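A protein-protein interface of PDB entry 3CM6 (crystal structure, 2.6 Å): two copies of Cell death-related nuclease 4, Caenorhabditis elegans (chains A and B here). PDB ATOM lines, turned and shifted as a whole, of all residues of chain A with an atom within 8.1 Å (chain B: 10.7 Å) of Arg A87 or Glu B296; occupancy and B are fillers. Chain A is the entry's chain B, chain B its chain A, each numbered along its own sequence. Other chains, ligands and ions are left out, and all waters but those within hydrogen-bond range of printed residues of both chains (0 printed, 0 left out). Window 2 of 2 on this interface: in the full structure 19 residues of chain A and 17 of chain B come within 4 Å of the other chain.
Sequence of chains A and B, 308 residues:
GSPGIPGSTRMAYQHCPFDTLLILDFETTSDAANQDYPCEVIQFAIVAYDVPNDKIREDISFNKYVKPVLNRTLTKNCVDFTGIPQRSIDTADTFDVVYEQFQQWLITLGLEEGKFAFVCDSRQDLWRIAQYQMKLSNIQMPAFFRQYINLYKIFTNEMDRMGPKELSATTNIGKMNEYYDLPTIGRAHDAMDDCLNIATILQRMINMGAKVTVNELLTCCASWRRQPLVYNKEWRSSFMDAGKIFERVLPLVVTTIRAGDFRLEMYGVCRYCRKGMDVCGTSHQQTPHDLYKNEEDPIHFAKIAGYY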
ATOM      1  N   TYR A  65     -37.619  18.886 -21.708  1.00  0.00           N
ATOM      2  CA  TYR A  65     -36.384  19.114 -22.406  1.00  0.00           C
ATOM      3  C   TYR A  65     -35.755  17.774 -22.757  1.00  0.00           C
ATOM      4  O   TYR A  65     -35.976  16.783 -22.062  1.00  0.00           O
ATOM      5  CB  TYR A  65     -35.452  19.936 -21.534  1.00  0.00           C
ATOM      6  CG  TYR A  65     -35.964  21.328 -21.380  1.00  0.00           C
ATOM      7  CD1 TYR A  65     -36.068  22.158 -22.492  1.00  0.00           C
ATOM      8  CD2 TYR A  65     -36.383  21.815 -20.136  1.00  0.00           C
ATOM      9  CE1 TYR A  65     -36.566  23.431 -22.380  1.00  0.00           C
ATOM     10  CE2 TYR A  65     -36.864  23.102 -20.010  1.00  0.00           C
ATOM     11  CZ  TYR A  65     -36.956  23.895 -21.135  1.00  0.00           C
ATOM     12  OH  TYR A  65     -37.436  25.178 -21.061  1.00  0.00           O
ATOM     13  N   LEU A  74     -25.542  23.629 -27.412  1.00  0.00           N
ATOM     14  CA  LEU A  74     -26.434  24.420 -28.235  1.00  0.00           C
ATOM     15  C   LEU A  74     -25.684  25.576 -28.857  1.00  0.00           C
ATOM     16  O   LEU A  74     -25.018  26.358 -28.191  1.00  0.00           O
ATOM     17  CB  LEU A  74     -27.632  24.928 -27.429  1.00  0.00           C
ATOM     18  CG  LEU A  74     -28.939  24.134 -27.402  1.00  0.00           C
ATOM     19  CD1 LEU A  74     -28.754  22.623 -27.384  1.00  0.00           C
ATOM     20  CD2 LEU A  74     -29.807  24.570 -26.226  1.00  0.00           C
ATOM     21  N   GLY A  83     -34.854  30.189 -27.312  1.00  0.00           N
ATOM     22  CA  GLY A  83     -34.936  30.667 -25.933  1.00  0.00           C
ATOM     23  C   GLY A  83     -34.472  29.619 -24.943  1.00  0.00           C
ATOM     24  O   GLY A  83     -34.355  29.900 -23.742  1.00  0.00           O
ATOM     25  N   ILE A  84     -34.199  28.403 -25.416  1.00  0.00           N
ATOM     26  CA  ILE A  84     -33.757  27.345 -24.512  1.00  0.00           C
ATOM     27  C   ILE A  84     -32.296  27.548 -24.053  1.00  0.00           C
ATOM     28  O   ILE A  84     -31.394  27.627 -24.897  1.00  0.00           O
ATOM     29  CB  ILE A  84     -33.915  25.970 -25.140  1.00  0.00           C
ATOM     30  CG1 ILE A  84     -35.345  25.813 -25.664  1.00  0.00           C
ATOM     31  CG2 ILE A  84     -33.519  24.870 -24.131  1.00  0.00           C
ATOM     32  CD1 ILE A  84     -35.628  24.508 -26.380  1.00  0.00           C
ATOM     33  N   PRO A  85     -32.059  27.642 -22.721  1.00  0.00           N
ATOM     34  CA  PRO A  85     -30.662  27.783 -22.241  1.00  0.00           C
ATOM     35  C   PRO A  85     -29.941  26.436 -22.064  1.00  0.00           C
ATOM     36  O   PRO A  85     -30.570  25.425 -21.730  1.00  0.00           O
ATOM     37  CB  PRO A  85     -30.837  28.454 -20.875  1.00  0.00           C
ATOM     38  CG  PRO A  85     -32.157  27.853 -20.357  1.00  0.00           C
ATOM     39  CD  PRO A  85     -33.033  27.642 -21.600  1.00  0.00           C
ATOM     40  N   GLN A  86     -28.625  26.441 -22.249  1.00  0.00           N
ATOM     41  CA  GLN A  86     -27.810  25.239 -22.101  1.00  0.00           C
ATOM     42  C   GLN A  86     -28.061  24.442 -20.804  1.00  0.00           C
ATOM     43  O   GLN A  86     -28.046  23.211 -20.827  1.00  0.00           O
ATOM     44  CB  GLN A  86     -26.318  25.570 -22.285  1.00  0.00           C
ATOM     45  CG  GLN A  86     -25.417  24.355 -22.383  1.00  0.00           C
ATOM     46  CD  GLN A  86     -25.707  23.491 -23.628  1.00  0.00           C
ATOM     47  OE1 GLN A  86     -25.841  24.013 -24.738  1.00  0.00           O
ATOM     48  NE2 GLN A  86     -25.795  22.178 -23.438  1.00  0.00           N
ATOM     49  N   ARG A  87     -28.310  25.114 -19.681  1.00  0.00           N
ATOM     50  CA  ARG A  87     -28.571  24.360 -18.418  1.00  0.00           C
ATOM     51  C   ARG A  87     -29.753  23.373 -18.469  1.00  0.00           C
ATOM     52  O   ARG A  87     -29.704  22.296 -17.858  1.00  0.00           O
ATOM     53  CB  ARG A  87     -28.710  25.277 -17.202  1.00  0.00           C
ATOM     54  CG  ARG A  87     -29.924  26.136 -17.182  1.00  0.00           C
ATOM     55  CD  ARG A  87     -29.819  27.195 -16.098  1.00  0.00           C
ATOM     56  NE  ARG A  87     -30.417  28.439 -16.568  1.00  0.00           N
ATOM     57  CZ  ARG A  87     -31.725  28.691 -16.549  1.00  0.00           C
ATOM     58  NH1 ARG A  87     -32.575  27.795 -16.040  1.00  0.00           N
ATOM     59  NH2 ARG A  87     -32.179  29.849 -17.030  1.00  0.00           N
ATOM     60  N   SER A  88     -30.799  23.737 -19.210  1.00  0.00           N
ATOM     61  CA  SER A  88     -31.999  22.920 -19.282  1.00  0.00           C
ATOM     62  C   SER A  88     -31.788  21.663 -20.105  1.00  0.00           C
ATOM     63  O   SER A  88     -32.427  20.636 -19.857  1.00  0.00           O
ATOM     64  CB  SER A  88     -33.163  23.743 -19.806  1.00  0.00           C
ATOM     65  OG  SER A  88     -33.406  24.819 -18.916  1.00  0.00           O
ATOM     66  N   ILE A  89     -30.873  21.719 -21.066  1.00  0.00           N
ATOM     67  CA  ILE A  89     -30.557  20.504 -21.802  1.00  0.00           C
ATOM     68  C   ILE A  89     -29.503  19.605 -21.101  1.00  0.00           C
ATOM     69  O   ILE A  89     -29.532  18.382 -21.263  1.00  0.00           O
ATOM     70  CB  ILE A  89     -30.281  20.760 -23.323  1.00  0.00           C
ATOM     71  CG1 ILE A  89     -28.808  20.907 -23.605  1.00  0.00           C
ATOM     72  CG2 ILE A  89     -31.086  21.941 -23.867  1.00  0.00           C
ATOM     73  CD1 ILE A  89     -28.153  19.602 -23.956  1.00  0.00           C
ATOM     74  N   ASP A  90     -28.609  20.197 -20.305  1.00  0.00           N
ATOM     75  CA  ASP A  90     -27.590  19.414 -19.572  1.00  0.00           C
ATOM     76  C   ASP A  90     -28.204  18.594 -18.421  1.00  0.00           C
ATOM     77  O   ASP A  90     -27.644  17.574 -17.999  1.00  0.00           O
ATOM     78  CB  ASP A  90     -26.447  20.296 -19.040  1.00  0.00           C
ATOM     79  CG  ASP A  90     -25.489  20.797 -20.143  1.00  0.00           C
ATOM     80  OD1 ASP A  90     -24.466  21.404 -19.779  1.00  0.00           O
ATOM     81  OD2 ASP A  90     -25.726  20.601 -21.358  1.00  0.00           O
ATOM     82  N   THR A  91     -29.358  19.014 -17.916  1.00  0.00           N
ATOM     83  CA  THR A  91     -30.047  18.210 -16.907  1.00  0.00           C
ATOM     84  C   THR A  91     -31.140  17.310 -17.496  1.00  0.00           C
ATOM     85  O   THR A  91     -31.720  16.510 -16.778  1.00  0.00           O
ATOM     86  CB  THR A  91     -30.626  19.088 -15.781  1.00  0.00           C
ATOM     87  OG1 THR A  91     -31.500  20.071 -16.349  1.00  0.00           O
ATOM     88  CG2 THR A  91     -29.490  19.809 -15.016  1.00  0.00           C
ATOM     89  N   ALA A  92     -31.404  17.435 -18.801  1.00  0.00           N
ATOM     90  CA  ALA A  92     -32.463  16.663 -19.479  1.00  0.00           C
ATOM     91  C   ALA A  92     -32.054  15.227 -19.736  1.00  0.00           C
ATOM     92  O   ALA A  92     -30.861  14.907 -19.742  1.00  0.00           O
ATOM     93  CB  ALA A  92     -32.849  17.326 -20.778  1.00  0.00           C
ATOM     94  N   ASN B  34     -20.125  31.943 -28.573  1.00  0.00           N
ATOM     95  CA  ASN B  34     -20.209  31.319 -27.265  1.00  0.00           C
ATOM     96  C   ASN B  34     -18.884  30.795 -26.738  1.00  0.00           C
ATOM     97  O   ASN B  34     -18.310  29.836 -27.264  1.00  0.00           O
ATOM     98  CB  ASN B  34     -21.265  30.223 -27.198  1.00  0.00           C
ATOM     99  CG  ASN B  34     -21.347  29.610 -25.829  1.00  0.00           C
ATOM    100  OD1 ASN B  34     -21.176  30.307 -24.819  1.00  0.00           O
ATOM    101  ND2 ASN B  34     -21.569  28.299 -25.769  1.00  0.00           N
ATOM    102  N   ASP B  36     -18.545  29.621 -23.530  1.00  0.00           N
ATOM    103  CA  ASP B  36     -18.804  28.455 -22.652  1.00  0.00           C
ATOM    104  C   ASP B  36     -18.962  27.199 -23.513  1.00  0.00           C
ATOM    105  O   ASP B  36     -20.025  26.584 -23.589  1.00  0.00           O
ATOM    106  CB  ASP B  36     -20.016  28.671 -21.738  1.00  0.00           C
ATOM    107  CG  ASP B  36     -20.162  27.587 -20.655  1.00  0.00           C
ATOM    108  OD1 ASP B  36     -19.365  26.616 -20.589  1.00  0.00           O
ATOM    109  OD2 ASP B  36     -21.100  27.713 -19.843  1.00  0.00           O
ATOM    110  N   TYR B 231     -16.581  37.159 -10.236  1.00  0.00           N
ATOM    111  CA  TYR B 231     -17.491  36.651 -11.273  1.00  0.00           C
ATOM    112  C   TYR B 231     -18.081  37.755 -12.159  1.00  0.00           C
ATOM    113  O   TYR B 231     -18.560  38.778 -11.665  1.00  0.00           O
ATOM    114  CB  TYR B 231     -18.607  35.784 -10.650  1.00  0.00           C
ATOM    115  CG  TYR B 231     -19.346  34.918 -11.661  1.00  0.00           C
ATOM    116  CD1 TYR B 231     -18.817  33.687 -12.079  1.00  0.00           C
ATOM    117  CD2 TYR B 231     -20.569  35.332 -12.209  1.00  0.00           C
ATOM    118  CE1 TYR B 231     -19.486  32.889 -13.019  1.00  0.00           C
ATOM    119  CE2 TYR B 231     -21.252  34.544 -13.149  1.00  0.00           C
ATOM    120  CZ  TYR B 231     -20.705  33.322 -13.552  1.00  0.00           C
ATOM    121  OH  TYR B 231     -21.375  32.541 -14.479  1.00  0.00           O
ATOM    122  N   LYS B 233     -20.981  38.065 -14.892  1.00  0.00           N
ATOM    123  CA  LYS B 233     -22.163  37.433 -15.501  1.00  0.00           C
ATOM    124  C   LYS B 233     -22.144  37.329 -17.033  1.00  0.00           C
ATOM    125  O   LYS B 233     -22.711  36.391 -17.593  1.00  0.00           O
ATOM    126  CB  LYS B 233     -23.453  38.125 -15.055  1.00  0.00           C
ATOM    127  CG  LYS B 233     -24.268  37.327 -14.034  1.00  0.00           C
ATOM    128  CD  LYS B 233     -24.165  37.916 -12.621  1.00  0.00           C
ATOM    129  CE  LYS B 233     -25.310  38.900 -12.366  1.00  0.00           C
ATOM    130  NZ  LYS B 233     -24.950  39.925 -11.335  1.00  0.00           N
ATOM    131  N   TRP B 235     -19.535  36.759 -19.053  1.00  0.00           N
ATOM    132  CA  TRP B 235     -18.253  36.186 -19.491  1.00  0.00           C
ATOM    133  C   TRP B 235     -18.306  35.379 -20.784  1.00  0.00           C
ATOM    134  O   TRP B 235     -17.342  35.360 -21.546  1.00  0.00           O
ATOM    135  CB  TRP B 235     -17.593  35.365 -18.382  1.00  0.00           C
ATOM    136  CG  TRP B 235     -18.283  34.089 -17.965  1.00  0.00           C
ATOM    137  CD1 TRP B 235     -19.182  33.938 -16.951  1.00  0.00           C
ATOM    138  CD2 TRP B 235     -18.073  32.781 -18.507  1.00  0.00           C
ATOM    139  NE1 TRP B 235     -19.558  32.623 -16.832  1.00  0.00           N
ATOM    140  CE2 TRP B 235     -18.893  31.889 -17.777  1.00  0.00           C
ATOM    141  CE3 TRP B 235     -17.280  32.274 -19.548  1.00  0.00           C
ATOM    142  CZ2 TRP B 235     -18.945  30.518 -18.051  1.00  0.00           C
ATOM    143  CZ3 TRP B 235     -17.326  30.910 -19.819  1.00  0.00           C
ATOM    144  CH2 TRP B 235     -18.148  30.048 -19.065  1.00  0.00           C
ATOM    145  N   ARG B 236     -19.437  34.729 -21.022  1.00  0.00           N
ATOM    146  CA  ARG B 236     -19.608  33.846 -22.166  1.00  0.00           C
ATOM    147  C   ARG B 236     -19.463  34.530 -23.515  1.00  0.00           C
ATOM    148  O   ARG B 236     -19.348  33.858 -24.526  1.00  0.00           O
ATOM    149  CB  ARG B 236     -20.936  33.100 -22.059  1.00  0.00           C
ATOM    150  CG  ARG B 236     -20.964  32.160 -20.877  1.00  0.00           C
ATOM    151  CD  ARG B 236     -22.339  31.679 -20.579  1.00  0.00           C
ATOM    152  NE  ARG B 236     -22.290  30.616 -19.584  1.00  0.00           N
ATOM    153  CZ  ARG B 236     -22.526  30.804 -18.290  1.00  0.00           C
ATOM    154  NH1 ARG B 236     -22.837  32.023 -17.859  1.00  0.00           N
ATOM    155  NH2 ARG B 236     -22.460  29.783 -17.428  1.00  0.00           N
ATOM    156  N   LEU B 291     -17.430  28.444  -7.658  1.00  0.00           N
ATOM    157  CA  LEU B 291     -17.962  28.668  -8.998  1.00  0.00           C
ATOM    158  C   LEU B 291     -19.062  27.664  -9.327  1.00  0.00           C
ATOM    159  O   LEU B 291     -19.884  27.887 -10.221  1.00  0.00           O
ATOM    160  CB  LEU B 291     -16.850  28.544 -10.037  1.00  0.00           C
ATOM    161  CG  LEU B 291     -15.938  29.726 -10.328  1.00  0.00           C
ATOM    162  CD1 LEU B 291     -14.976  29.325 -11.431  1.00  0.00           C
ATOM    163  CD2 LEU B 291     -16.735  30.962 -10.731  1.00  0.00           C
ATOM    164  N   TYR B 292     -19.065  26.562  -8.591  1.00  0.00           N
ATOM    165  CA  TYR B 292     -19.934  25.436  -8.879  1.00  0.00           C
ATOM    166  C   TYR B 292     -21.211  25.427  -8.010  1.00  0.00           C
ATOM    167  O   TYR B 292     -21.835  24.379  -7.802  1.00  0.00           O
ATOM    168  CB  TYR B 292     -19.140  24.136  -8.695  1.00  0.00           C
ATOM    169  CG  TYR B 292     -17.959  23.952  -9.634  1.00  0.00           C
ATOM    170  CD1 TYR B 292     -17.890  24.612 -10.858  1.00  0.00           C
ATOM    171  CD2 TYR B 292     -16.925  23.084  -9.304  1.00  0.00           C
ATOM    172  CE1 TYR B 292     -16.812  24.420 -11.712  1.00  0.00           C
ATOM    173  CE2 TYR B 292     -15.853  22.882 -10.159  1.00  0.00           C
ATOM    174  CZ  TYR B 292     -15.805  23.549 -11.354  1.00  0.00           C
ATOM    175  OH  TYR B 292     -14.740  23.345 -12.190  1.00  0.00           O
ATOM    176  N   LYS B 293     -21.603  26.602  -7.524  1.00  0.00           N
ATOM    177  CA  LYS B 293     -22.668  26.689  -6.532  1.00  0.00           C
ATOM    178  C   LYS B 293     -23.982  27.247  -7.065  1.00  0.00           C
ATOM    179  O   LYS B 293     -25.035  26.949  -6.514  1.00  0.00           O
ATOM    180  CB  LYS B 293     -22.187  27.433  -5.277  1.00  0.00           C
ATOM    181  CG  LYS B 293     -21.733  26.470  -4.165  1.00  0.00           C
ATOM    182  CD  LYS B 293     -20.447  26.900  -3.433  1.00  0.00           C
ATOM    183  CE  LYS B 293     -20.587  28.213  -2.648  1.00  0.00           C
ATOM    184  NZ  LYS B 293     -19.264  28.724  -2.131  1.00  0.00           N
ATOM    185  N   ASN B 294     -23.923  28.021  -8.145  1.00  0.00           N
ATOM    186  CA  ASN B 294     -25.117  28.632  -8.735  1.00  0.00           C
ATOM    187  C   ASN B 294     -25.683  27.821  -9.911  1.00  0.00           C
ATOM    188  O   ASN B 294     -25.467  28.175 -11.079  1.00  0.00           O
ATOM    189  CB  ASN B 294     -24.822  30.088  -9.162  1.00  0.00           C
ATOM    190  CG  ASN B 294     -26.056  30.815  -9.725  1.00  0.00           C
ATOM    191  OD1 ASN B 294     -27.205  30.429  -9.473  1.00  0.00           O
ATOM    192  ND2 ASN B 294     -25.814  31.871 -10.493  1.00  0.00           N
ATOM    193  N   GLU B 295     -26.427  26.756  -9.605  1.00  0.00           N
ATOM    194  CA  GLU B 295     -27.008  25.889 -10.645  1.00  0.00           C
ATOM    195  C   GLU B 295     -28.175  26.518 -11.453  1.00  0.00           C
ATOM    196  O   GLU B 295     -28.950  25.813 -12.107  1.00  0.00           O
ATOM    197  CB  GLU B 295     -27.362  24.507 -10.077  1.00  0.00           C
ATOM    198  CG  GLU B 295     -28.435  24.509  -8.997  1.00  0.00           C
ATOM    199  CD  GLU B 295     -28.111  23.545  -7.852  1.00  0.00           C
ATOM    200  OE1 GLU B 295     -27.013  23.694  -7.249  1.00  0.00           O
ATOM    201  OE2 GLU B 295     -28.950  22.652  -7.554  1.00  0.00           O
ATOM    202  N   GLU B 296     -28.268  27.847 -11.411  1.00  0.00           N
ATOM    203  CA  GLU B 296     -29.139  28.620 -12.295  1.00  0.00           C
ATOM    204  C   GLU B 296     -28.269  29.363 -13.321  1.00  0.00           C
ATOM    205  O   GLU B 296     -28.785  29.959 -14.279  1.00  0.00           O
ATOM    206  CB  GLU B 296     -29.988  29.611 -11.473  1.00  0.00           C
ATOM    207  CG  GLU B 296     -31.319  30.071 -12.124  1.00  0.00           C
ATOM    208  CD  GLU B 296     -32.407  28.978 -12.139  1.00  0.00           C
ATOM    209  OE1 GLU B 296     -32.616  28.295 -11.103  1.00  0.00           O
ATOM    210  OE2 GLU B 296     -33.065  28.811 -13.191  1.00  0.00           O
ATOM    211  N   ASP B 297     -26.950  29.347 -13.086  1.00  0.00           N
ATOM    212  CA  ASP B 297     -25.945  29.838 -14.055  1.00  0.00           C
ATOM    213  C   ASP B 297     -24.737  28.877 -14.172  1.00  0.00           C
ATOM    214  O   ASP B 297     -23.596  29.271 -13.926  1.00  0.00           O
ATOM    215  CB  ASP B 297     -25.481  31.255 -13.697  1.00  0.00           C
ATOM    216  CG  ASP B 297     -24.796  31.960 -14.867  1.00  0.00           C
ATOM    217  OD1 ASP B 297     -24.387  33.140 -14.725  1.00  0.00           O
ATOM    218  OD2 ASP B 297     -24.676  31.337 -15.941  1.00  0.00           O
ATOM    219  N   PRO B 298     -24.975  27.618 -14.581  1.00  0.00           N
ATOM    220  CA  PRO B 298     -23.854  26.679 -14.491  1.00  0.00           C
ATOM    221  C   PRO B 298     -22.842  26.879 -15.626  1.00  0.00           C
ATOM    222  O   PRO B 298     -23.133  27.559 -16.621  1.00  0.00           O
ATOM    223  CB  PRO B 298     -24.527  25.290 -14.577  1.00  0.00           C
ATOM    224  CG  PRO B 298     -26.013  25.557 -14.779  1.00  0.00           C
ATOM    225  CD  PRO B 298     -26.165  26.988 -15.178  1.00  0.00           C
ATOM    226  N   ILE B 299     -21.649  26.323 -15.438  1.00  0.00           N
ATOM    227  CA  ILE B 299     -20.573  26.416 -16.420  1.00  0.00           C
ATOM    228  C   ILE B 299     -20.649  25.136 -17.223  1.00  0.00           C
ATOM    229  O   ILE B 299     -20.297  24.048 -16.738  1.00  0.00           O
ATOM    230  CB  ILE B 299     -19.168  26.491 -15.753  1.00  0.00           C
ATOM    231  CG1 ILE B 299     -19.104  27.558 -14.641  1.00  0.00           C
ATOM    232  CG2 ILE B 299     -18.069  26.650 -16.816  1.00  0.00           C
ATOM    233  CD1 ILE B 299     -19.801  28.880 -14.970  1.00  0.00           C
ATOM    234  N   HIS B 300     -21.138  25.275 -18.451  1.00  0.00           N
ATOM    235  CA  HIS B 300     -21.378  24.135 -19.307  1.00  0.00           C
ATOM    236  C   HIS B 300     -20.094  23.323 -19.558  1.00  0.00           C
ATOM    237  O   HIS B 300     -20.109  22.096 -19.403  1.00  0.00           O
ATOM    238  CB  HIS B 300     -22.072  24.578 -20.601  1.00  0.00           C
ATOM    239  CG  HIS B 300     -22.074  23.540 -21.679  1.00  0.00           C
ATOM    240  ND1 HIS B 300     -22.719  22.331 -21.547  1.00  0.00           N
ATOM    241  CD2 HIS B 300     -21.494  23.528 -22.903  1.00  0.00           C
ATOM    242  CE1 HIS B 300     -22.543  21.620 -22.647  1.00  0.00           C
ATOM    243  NE2 HIS B 300     -21.800  22.324 -23.483  1.00  0.00           N
ATOM    244  N   PHE B 301     -18.987  23.987 -19.899  1.00  0.00           N
ATOM    245  CA  PHE B 301     -17.772  23.238 -20.235  1.00  0.00           C
ATOM    246  C   PHE B 301     -17.250  22.424 -19.070  1.00  0.00           C
ATOM    247  O   PHE B 301     -16.790  21.294 -19.260  1.00  0.00           O
ATOM    248  CB  PHE B 301     -16.695  24.083 -20.955  1.00  0.00           C
ATOM    249  CG  PHE B 301     -15.873  24.978 -20.064  1.00  0.00           C
ATOM    250  CD1 PHE B 301     -16.094  26.345 -20.050  1.00  0.00           C
ATOM    251  CD2 PHE B 301     -14.832  24.468 -19.290  1.00  0.00           C
ATOM    252  CE1 PHE B 301     -15.310  27.194 -19.243  1.00  0.00           C
ATOM    253  CE2 PHE B 301     -14.060  25.297 -18.477  1.00  0.00           C
ATOM    254  CZ  PHE B 301     -14.297  26.661 -18.453  1.00  0.00           C
ATOM    255  N   LYS B 303     -19.220  21.227 -16.610  1.00  0.00           N
ATOM    256  CA  LYS B 303     -20.181  20.124 -16.474  1.00  0.00           C
ATOM    257  C   LYS B 303     -20.022  18.949 -17.445  1.00  0.00           C
ATOM    258  O   LYS B 303     -19.932  17.818 -16.980  1.00  0.00           O
ATOM    259  CB  LYS B 303     -21.642  20.601 -16.427  1.00  0.00           C
ATOM    260  CG  LYS B 303     -22.268  20.376 -15.030  1.00  0.00           C
ATOM    261  CD  LYS B 303     -23.788  20.231 -15.084  1.00  0.00           C
ATOM    262  CE  LYS B 303     -24.246  18.760 -15.327  1.00  0.00           C
ATOM    263  NZ  LYS B 303     -25.736  18.594 -15.151  1.00  0.00           N
ATOM    264  N   ILE B 304     -19.979  19.185 -18.764  1.00  0.00           N
ATOM    265  CA  ILE B 304     -19.834  18.049 -19.726  1.00  0.00           C
ATOM    266  C   ILE B 304     -18.526  17.266 -19.521  1.00  0.00           C
ATOM    267  O   ILE B 304     -18.436  16.089 -19.853  1.00  0.00           O
ATOM    268  CB  ILE B 304     -19.882  18.485 -21.214  1.00  0.00           C
ATOM    269  CG1 ILE B 304     -19.864  19.992 -21.303  1.00  0.00           C
ATOM    270  CG2 ILE B 304     -21.105  17.911 -21.979  1.00  0.00           C
ATOM    271  CD1 ILE B 304     -18.810  20.480 -22.173  1.00  0.00           C
ATOM    272  N   TYR B 308     -17.560  18.876 -12.320  1.00  0.00           N
ATOM    273  CA  TYR B 308     -18.593  18.810 -11.282  1.00  0.00           C
ATOM    274  C   TYR B 308     -19.926  18.447 -11.911  1.00  0.00           C
ATOM    275  O   TYR B 308     -19.988  18.033 -13.074  1.00  0.00           O
ATOM    276  CB  TYR B 308     -18.737  20.144 -10.537  1.00  0.00           C
ATOM    277  CG  TYR B 308     -19.491  21.262 -11.264  1.00  0.00           C
ATOM    278  CD1 TYR B 308     -19.052  21.756 -12.503  1.00  0.00           C
ATOM    279  CD2 TYR B 308     -20.615  21.858 -10.683  1.00  0.00           C
ATOM    280  CE1 TYR B 308     -19.722  22.792 -13.152  1.00  0.00           C
ATOM    281  CE2 TYR B 308     -21.293  22.913 -11.327  1.00  0.00           C
ATOM    282  CZ  TYR B 308     -20.835  23.368 -12.559  1.00  0.00           C
ATOM    283  OH  TYR B 308     -21.484  24.406 -13.197  1.00  0.00           O
ATOM    284  OXT TYR B 308     -20.970  18.595 -11.270  1.00  0.00           O
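ND1 of His B300 sits at hydrogen-bond distance from OD1 of Asp A90. The guanidinium group (NH1) of Arg A87 lies within salt-bridge range of the side-chain carboxylate (OE2) of Glu B296.
OG1 of Thr A91 lies within hydrogen-bond range of O of Arg A87. NH2 of Arg B236 lies within hydrogen-bond range of O of Pro B298 (2.5 Å). OD2 of Asp A90 sits at hydrogen-bond distance from NE2 of Gln A86 (2.6 Å). The backbone NH of His B300 sits at hydrogen-bond distance from the side-chain carboxylate of Asp B36, at 2.8 Å. The side-chain amide oxygen of Asn B294 lies close to the backbone NH of Glu B296 (3.4 Å). The backbone NH of Leu A74 sits at hydrogen-bond distance from the side-chain amide oxygen of Gln A86, at 2.7 Å.
Among the printed residues, pairs that only touch across the chains: Gln A86 with His B300 (3.4 Å), Asp A90 with Lys B303 (3.6 Å), Arg A87 with Pro B298 (3.6 Å) and Thr A91 with Lys B303 (3.9 Å).
No residue of chain B comes within 4 Å of Pro A85. Of chain B, only His B300 (3.4 Å) comes within 4 Å of Gln A86. Arg A87 touches just these residues of chain B: Glu B296 (3.1 Å) and Pro B298 (3.6 Å). Of chain B, only Lys B303 (3.9 Å) comes within 4 Å of Thr A91. Of the printed residues of chain A, Glu B296 touches Arg A87 (3.1 Å). Printed residues of chain A within 4 Å of Pro B298: Arg A87 (3.6 Å). Printed residues of chain A within 4 Å of His B300: Gln A86 (3.4 Å) and Asp A90 (2.7 Å). The nearest residue of chain B that does not touch Arg A87 is Glu B295 (4.3 Å). The nearest residue of chain A that does not touch Glu B296 is Ser A88 (7.0 Å).
Of the 20 printed residues of chain B, 4 touch a printed residue of chain A. Printed residues of chain B that touch a printed residue of chain A: Glu B296, Pro B298, His B300 and Lys B303. Among the printed residues, Asp or Glu carboxylates within 4 Å of a Lys or Arg side-chain nitrogen of the other chain: Arg A87 with Glu B296.
No position is printed for both chains. Of the 6 pairs that touch across the chains among the printed residues, none has its exchanged pair printed and touching as well.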
